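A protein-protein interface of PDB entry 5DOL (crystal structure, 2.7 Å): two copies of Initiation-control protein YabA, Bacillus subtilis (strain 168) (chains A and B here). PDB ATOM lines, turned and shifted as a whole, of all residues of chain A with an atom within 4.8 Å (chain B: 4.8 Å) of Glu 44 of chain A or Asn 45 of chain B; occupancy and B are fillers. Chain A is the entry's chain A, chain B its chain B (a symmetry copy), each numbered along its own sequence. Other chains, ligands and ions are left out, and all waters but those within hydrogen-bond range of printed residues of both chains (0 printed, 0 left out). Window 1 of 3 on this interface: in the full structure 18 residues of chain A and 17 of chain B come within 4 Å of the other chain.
Glu 44 of chain A touches just these residues of chain B: Asn 45 and Arg 49. Asn 45 of chain B touches just these residues of chain A: Leu 41 (3.2 Å), Glu 44 (3.3 Å), Asn 45 (2.9 Å) and Leu 48 (3.8 Å). Of the printed residues of chain B, Leu 48 of chain A touches Asn 45 (3.8 Å), Leu 48 (3.98 Å) and Arg 49 (3.99 Å). Of the printed residues of chain B, Asn 45 of chain A touches Glu 44, Asn 45 and Leu 48. Of the printed residues of chain A, Leu 41 of chain B touches Leu 41 (3.7 Å) and Gln 42 (3.7 Å). Of the printed residues of chain A, Arg 49 of chain B touches Glu 44 and Leu 48. Of the printed residues of chain B, Gln 42 of chain A touches Leu 41. Lys 46 of chain A touches none of the printed residues of chain B. Leu 43 of chain A touches none of the printed residues of chain B. The nearest printed residue of chain A that does not touch Asn 45 of chain B is Gln 42 of chain A (5.3 Å). The nearest printed residue of chain A that does not touch Glu 44 of chain B is Leu 48 of chain A (5.9 Å).
Along chain A the printed residues that touch a printed residue of chain B span positions 41 to 48.
The side-chain amide nitrogen of Asn 45 of chain B sits at hydrogen-bond distance from the backbone carbonyl oxygen of Leu 41 of chain A. ND2 of Asn 45 of chain B sits at hydrogen-bond distance from OE1 of Glu 44 of chain A. The guanidinium group (NH2) of Arg 49 of chain B is in salt-bridge range of the side-chain carboxylate (OE2) of Glu 44 of chain A, at 2.6 Å. The side-chain amide nitrogen (ND2) of Asn 45 of chain A lies close to the side-chain carboxylate (OE1) of Glu 44 of chain B, at 3.4 Å. The side-chain amide nitrogen (ND2) of Asn 45 of chain A is in hydrogen-bond range of the side-chain amide oxygen (OD1) of Asn 45 of chain B (2.9 Å).
O of Leu 41 of chain B lies close to OD1 of Asn 45 of chain B (3.2 Å).
Leu 41 of chain A touches Gln 42 of chain B, and with the chains exchanged Gln 42 of chain A touches Leu 41 of chain B. Asn 45 of chain A touches its own counterpart, Asn 45 of chain B. Asn 45 of chain A touches Leu 48 of chain B, and with the chains exchanged Leu 48 of chain A touches Asn 45 of chain B. Leu 48 of chain B touches its own counterpart, Leu 48 of chain A. Positions printed for both chains: 40, 41, 42, 43, 44, 45, 46, 47 and 48.
Among the printed residues, pairs that only touch across the chains: Leu 41 of chain A with Leu 41 of chain B (3.7 Å), Leu 41 of chain A with Gln 42 of chain B (3.9 Å), Gln 42 of chain A with Leu 41 of chain B (3.7 Å), Asn 45 of chain A with Leu 48 of chain B (3.3 Å), Leu 48 of chain A with Asn 45 of chain B (3.8 Å), Leu 48 of chain A with Leu 48 of chain B (3.98 Å) and Leu 48 of chain A with Arg 49 of chain B (3.99 Å).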
ATOM      1  N   HIS A  40      -9.454  14.388 -28.148  1.00  0.00           N
ATOM      2  CA  HIS A  40      -8.865  13.265 -27.437  1.00  0.00           C
ATOM      3  C   HIS A  40      -8.952  13.482 -25.921  1.00  0.00           C
ATOM      4  O   HIS A  40      -9.225  12.554 -25.158  1.00  0.00           O
ATOM      5  CB  HIS A  40      -7.414  13.068 -27.886  1.00  0.00           C
ATOM      6  CG  HIS A  40      -7.245  12.993 -29.376  1.00  0.00           C
ATOM      7  ND1 HIS A  40      -6.069  13.333 -30.011  1.00  0.00           N
ATOM      8  CD2 HIS A  40      -8.103  12.618 -30.354  1.00  0.00           C
ATOM      9  CE1 HIS A  40      -6.209  13.169 -31.314  1.00  0.00           C
ATOM     10  NE2 HIS A  40      -7.433  12.731 -31.550  1.00  0.00           N
ATOM     11  N   LEU A  41      -8.709  14.718 -25.491  1.00  0.00           N
ATOM     12  CA  LEU A  41      -8.783  15.038 -24.067  1.00  0.00           C
ATOM     13  C   LEU A  41     -10.180  14.825 -23.518  1.00  0.00           C
ATOM     14  O   LEU A  41     -10.347  14.345 -22.392  1.00  0.00           O
ATOM     15  CB  LEU A  41      -8.347  16.475 -23.814  1.00  0.00           C
ATOM     16  CG  LEU A  41      -6.837  16.700 -23.862  1.00  0.00           C
ATOM     17  CD1 LEU A  41      -6.519  18.169 -23.694  1.00  0.00           C
ATOM     18  CD2 LEU A  41      -6.159  15.862 -22.783  1.00  0.00           C
ATOM     19  N   GLN A  42     -11.189  15.186 -24.306  1.00  0.00           N
ATOM     20  CA  GLN A  42     -12.575  14.993 -23.883  1.00  0.00           C
ATOM     21  C   GLN A  42     -12.890  13.515 -23.769  1.00  0.00           C
ATOM     22  O   GLN A  42     -13.492  13.089 -22.780  1.00  0.00           O
ATOM     23  CB  GLN A  42     -13.550  15.670 -24.845  1.00  0.00           C
ATOM     24  CG  GLN A  42     -13.616  17.184 -24.703  1.00  0.00           C
ATOM     25  CD  GLN A  42     -14.493  17.823 -25.761  1.00  0.00           C
ATOM     26  OE1 GLN A  42     -15.125  17.131 -26.559  1.00  0.00           O
ATOM     27  NE2 GLN A  42     -14.532  19.150 -25.776  1.00  0.00           N
ATOM     28  N   LEU A  43     -12.470  12.731 -24.766  1.00  0.00           N
ATOM     29  CA  LEU A  43     -12.690  11.275 -24.714  1.00  0.00           C
ATOM     30  C   LEU A  43     -12.008  10.601 -23.514  1.00  0.00           C
ATOM     31  O   LEU A  43     -12.613   9.777 -22.807  1.00  0.00           O
ATOM     32  CB  LEU A  43     -12.214  10.623 -26.004  1.00  0.00           C
ATOM     33  CG  LEU A  43     -13.084  10.888 -27.231  1.00  0.00           C
ATOM     34  CD1 LEU A  43     -12.435  10.302 -28.460  1.00  0.00           C
ATOM     35  CD2 LEU A  43     -14.471  10.305 -27.032  1.00  0.00           C
ATOM     36  N   GLU A  44     -10.747  10.958 -23.296  1.00  0.00           N
ATOM     37  CA  GLU A  44      -9.970  10.472 -22.164  1.00  0.00           C
ATOM     38  C   GLU A  44     -10.658  10.838 -20.857  1.00  0.00           C
ATOM     39  O   GLU A  44     -10.761  10.015 -19.948  1.00  0.00           O
ATOM     40  CB  GLU A  44      -8.552  11.051 -22.194  1.00  0.00           C
ATOM     41  CG  GLU A  44      -7.633  10.555 -21.085  1.00  0.00           C
ATOM     42  CD  GLU A  44      -6.282  11.253 -21.081  1.00  0.00           C
ATOM     43  OE1 GLU A  44      -6.078  12.178 -21.901  1.00  0.00           O
ATOM     44  OE2 GLU A  44      -5.417  10.878 -20.257  1.00  0.00           O
ATOM     45  N   ASN A  45     -11.135  12.076 -20.775  1.00  0.00           N
ATOM     46  CA  ASN A  45     -11.845  12.550 -19.595  1.00  0.00           C
ATOM     47  C   ASN A  45     -13.093  11.717 -19.331  1.00  0.00           C
ATOM     48  O   ASN A  45     -13.309  11.259 -18.208  1.00  0.00           O
ATOM     49  CB  ASN A  45     -12.210  14.027 -19.753  1.00  0.00           C
ATOM     50  CG  ASN A  45     -12.950  14.580 -18.551  1.00  0.00           C
ATOM     51  OD1 ASN A  45     -14.180  14.612 -18.528  1.00  0.00           O
ATOM     52  ND2 ASN A  45     -12.203  15.020 -17.545  1.00  0.00           N
ATOM     53  N   LYS A  46     -13.900  11.512 -20.373  1.00  0.00           N
ATOM     54  CA  LYS A  46     -15.069  10.638 -20.287  1.00  0.00           C
ATOM     55  C   LYS A  46     -14.700   9.273 -19.725  1.00  0.00           C
ATOM     56  O   LYS A  46     -15.334   8.786 -18.776  1.00  0.00           O
ATOM     57  CB  LYS A  46     -15.729  10.453 -21.659  1.00  0.00           C
ATOM     58  CG  LYS A  46     -16.558  11.624 -22.153  1.00  0.00           C
ATOM     59  N   HIS A  47     -13.673   8.651 -20.307  1.00  0.00           N
ATOM     60  CA  HIS A  47     -13.327   7.302 -19.865  1.00  0.00           C
ATOM     61  C   HIS A  47     -12.824   7.259 -18.427  1.00  0.00           C
ATOM     62  O   HIS A  47     -13.096   6.308 -17.704  1.00  0.00           O
ATOM     63  CB  HIS A  47     -12.273   6.656 -20.752  1.00  0.00           C
ATOM     64  CG  HIS A  47     -11.847   5.314 -20.251  1.00  0.00           C
ATOM     65  ND1 HIS A  47     -10.774   5.144 -19.406  1.00  0.00           N
ATOM     66  CD2 HIS A  47     -12.400   4.091 -20.414  1.00  0.00           C
ATOM     67  CE1 HIS A  47     -10.661   3.865 -19.095  1.00  0.00           C
ATOM     68  NE2 HIS A  47     -11.634   3.204 -19.692  1.00  0.00           N
ATOM     69  N   LEU A  48     -12.060   8.267 -18.024  1.00  0.00           N
ATOM     70  CA  LEU A  48     -11.518   8.283 -16.676  1.00  0.00           C
ATOM     71  C   LEU A  48     -12.652   8.497 -15.686  1.00  0.00           C
ATOM     72  O   LEU A  48     -12.660   7.907 -14.607  1.00  0.00           O
ATOM     73  CB  LEU A  48     -10.444   9.360 -16.535  1.00  0.00           C
ATOM     74  CG  LEU A  48      -9.193   9.109 -17.397  1.00  0.00           C
ATOM     75  CD1 LEU A  48      -8.195  10.242 -17.260  1.00  0.00           C
ATOM     76  CD2 LEU A  48      -8.549   7.771 -17.050  1.00  0.00           C
ATOM     77  N   HIS B  40      -7.635  23.065 -18.881  1.00  0.00           N
ATOM     78  CA  HIS B  40      -8.557  22.523 -17.877  1.00  0.00           C
ATOM     79  C   HIS B  40      -8.661  21.012 -18.012  1.00  0.00           C
ATOM     80  O   HIS B  40      -8.478  20.282 -17.038  1.00  0.00           O
ATOM     81  CB  HIS B  40      -9.950  23.146 -18.002  1.00  0.00           C
ATOM     82  CG  HIS B  40     -10.051  24.536 -17.456  1.00  0.00           C
ATOM     83  ND1 HIS B  40     -11.254  25.123 -17.129  1.00  0.00           N
ATOM     84  CD2 HIS B  40      -9.097  25.458 -17.179  1.00  0.00           C
ATOM     85  CE1 HIS B  40     -11.038  26.345 -16.674  1.00  0.00           C
ATOM     86  NE2 HIS B  40      -9.738  26.572 -16.696  1.00  0.00           N
ATOM     87  N   LEU B  41      -8.950  20.549 -19.225  1.00  0.00           N
ATOM     88  CA  LEU B  41      -8.999  19.118 -19.496  1.00  0.00           C
ATOM     89  C   LEU B  41      -7.709  18.414 -19.101  1.00  0.00           C
ATOM     90  O   LEU B  41      -7.741  17.328 -18.529  1.00  0.00           O
ATOM     91  CB  LEU B  41      -9.288  18.867 -20.971  1.00  0.00           C
ATOM     92  CG  LEU B  41     -10.763  19.009 -21.328  1.00  0.00           C
ATOM     93  CD1 LEU B  41     -10.964  18.895 -22.826  1.00  0.00           C
ATOM     94  CD2 LEU B  41     -11.570  17.956 -20.578  1.00  0.00           C
ATOM     95  N   GLN B  42      -6.573  19.034 -19.408  1.00  0.00           N
ATOM     96  CA  GLN B  42      -5.284  18.447 -19.068  1.00  0.00           C
ATOM     97  C   GLN B  42      -5.158  18.198 -17.573  1.00  0.00           C
ATOM     98  O   GLN B  42      -5.008  17.041 -17.134  1.00  0.00           O
ATOM     99  CB  GLN B  42      -4.144  19.338 -19.552  1.00  0.00           C
ATOM    100  CG  GLN B  42      -3.843  19.189 -21.037  1.00  0.00           C
ATOM    101  CD  GLN B  42      -2.801  20.173 -21.529  1.00  0.00           C
ATOM    102  OE1 GLN B  42      -2.539  21.192 -20.888  1.00  0.00           O
ATOM    103  NE2 GLN B  42      -2.198  19.871 -22.673  1.00  0.00           N
ATOM    104  N   LEU B  43      -5.238  19.270 -16.782  1.00  0.00           N
ATOM    105  CA  LEU B  43      -5.042  19.104 -15.336  1.00  0.00           C
ATOM    106  C   LEU B  43      -6.113  18.194 -14.721  1.00  0.00           C
ATOM    107  O   LEU B  43      -5.826  17.374 -13.834  1.00  0.00           O
ATOM    108  CB  LEU B  43      -5.013  20.465 -14.629  1.00  0.00           C
ATOM    109  CG  LEU B  43      -6.068  21.529 -14.936  1.00  0.00           C
ATOM    110  CD1 LEU B  43      -7.292  21.372 -14.046  1.00  0.00           C
ATOM    111  CD2 LEU B  43      -5.468  22.920 -14.780  1.00  0.00           C
ATOM    112  N   GLU B  44      -7.339  18.328 -15.224  1.00  0.00           N
ATOM    113  CA  GLU B  44      -8.475  17.511 -14.799  1.00  0.00           C
ATOM    114  C   GLU B  44      -8.184  16.028 -14.975  1.00  0.00           C
ATOM    115  O   GLU B  44      -8.391  15.238 -14.059  1.00  0.00           O
ATOM    116  CB  GLU B  44      -9.723  17.903 -15.594  1.00  0.00           C
ATOM    117  CG  GLU B  44     -11.037  17.307 -15.127  1.00  0.00           C
ATOM    118  CD  GLU B  44     -12.214  17.871 -15.909  1.00  0.00           C
ATOM    119  OE1 GLU B  44     -12.004  18.360 -17.041  1.00  0.00           O
ATOM    120  OE2 GLU B  44     -13.347  17.839 -15.391  1.00  0.00           O
ATOM    121  N   ASN B  45      -7.700  15.656 -16.156  1.00  0.00           N
ATOM    122  CA  ASN B  45      -7.356  14.266 -16.426  1.00  0.00           C
ATOM    123  C   ASN B  45      -6.153  13.806 -15.602  1.00  0.00           C
ATOM    124  O   ASN B  45      -6.073  12.639 -15.210  1.00  0.00           O
ATOM    125  CB  ASN B  45      -7.091  14.059 -17.918  1.00  0.00           C
ATOM    126  CG  ASN B  45      -8.348  14.227 -18.761  1.00  0.00           C
ATOM    127  OD1 ASN B  45      -9.397  14.628 -18.255  1.00  0.00           O
ATOM    128  ND2 ASN B  45      -8.244  13.932 -20.051  1.00  0.00           N
ATOM    129  N   LYS B  46      -5.223  14.722 -15.332  1.00  0.00           N
ATOM    130  CA  LYS B  46      -4.101  14.394 -14.453  1.00  0.00           C
ATOM    131  C   LYS B  46      -4.592  13.967 -13.064  1.00  0.00           C
ATOM    132  O   LYS B  46      -4.225  12.894 -12.544  1.00  0.00           O
ATOM    133  CB  LYS B  46      -3.151  15.586 -14.336  1.00  0.00           C
ATOM    134  CG  LYS B  46      -2.029  15.382 -13.335  1.00  0.00           C
ATOM    135  N   HIS B  47      -5.434  14.808 -12.470  1.00  0.00           N
ATOM    136  CA  HIS B  47      -5.992  14.519 -11.155  1.00  0.00           C
ATOM    137  C   HIS B  47      -6.892  13.279 -11.172  1.00  0.00           C
ATOM    138  O   HIS B  47      -6.925  12.502 -10.207  1.00  0.00           O
ATOM    139  CB  HIS B  47      -6.757  15.734 -10.637  1.00  0.00           C
ATOM    140  CG  HIS B  47      -5.875  16.891 -10.297  1.00  0.00           C
ATOM    141  ND1 HIS B  47      -4.500  16.798 -10.282  1.00  0.00           N
ATOM    142  CD2 HIS B  47      -6.166  18.172  -9.961  1.00  0.00           C
ATOM    143  CE1 HIS B  47      -3.983  17.966  -9.950  1.00  0.00           C
ATOM    144  NE2 HIS B  47      -4.974  18.817  -9.750  1.00  0.00           N
ATOM    145  N   LEU B  48      -7.615  13.096 -12.273  1.00  0.00           N
ATOM    146  CA  LEU B  48      -8.445  11.909 -12.449  1.00  0.00           C
ATOM    147  C   LEU B  48      -7.577  10.658 -12.428  1.00  0.00           C
ATOM    148  O   LEU B  48      -7.972   9.625 -11.883  1.00  0.00           O
ATOM    149  CB  LEU B  48      -9.240  11.985 -13.755  1.00  0.00           C
ATOM    150  CG  LEU B  48     -10.483  12.882 -13.752  1.00  0.00           C
ATOM    151  CD1 LEU B  48     -11.029  13.050 -15.157  1.00  0.00           C
ATOM    152  CD2 LEU B  48     -11.550  12.325 -12.827  1.00  0.00           C
ATOM    153  N   ARG B  49      -6.388  10.757 -13.015  1.00  0.00           N
ATOM    154  CA  ARG B  49      -5.434   9.655 -12.979  1.00  0.00           C
ATOM    155  C   ARG B  49      -4.865   9.468 -11.575  1.00  0.00           C
ATOM    156  O   ARG B  49      -4.555   8.344 -11.177  1.00  0.00           O
ATOM    157  CB  ARG B  49      -4.306   9.880 -13.986  1.00  0.00           C
ATOM    158  CG  ARG B  49      -4.716   9.595 -15.416  1.00  0.00           C
ATOM    159  CD  ARG B  49      -3.571   9.804 -16.386  1.00  0.00           C
ATOM    160  NE  ARG B  49      -4.027   9.665 -17.764  1.00  0.00           N
ATOM    161  CZ  ARG B  49      -4.103   8.506 -18.412  1.00  0.00           C
ATOM    162  NH1 ARG B  49      -3.744   7.380 -17.813  1.00  0.00           N
ATOM    163  NH2 ARG B  49      -4.536   8.477 -19.662  1.00  0.00           N
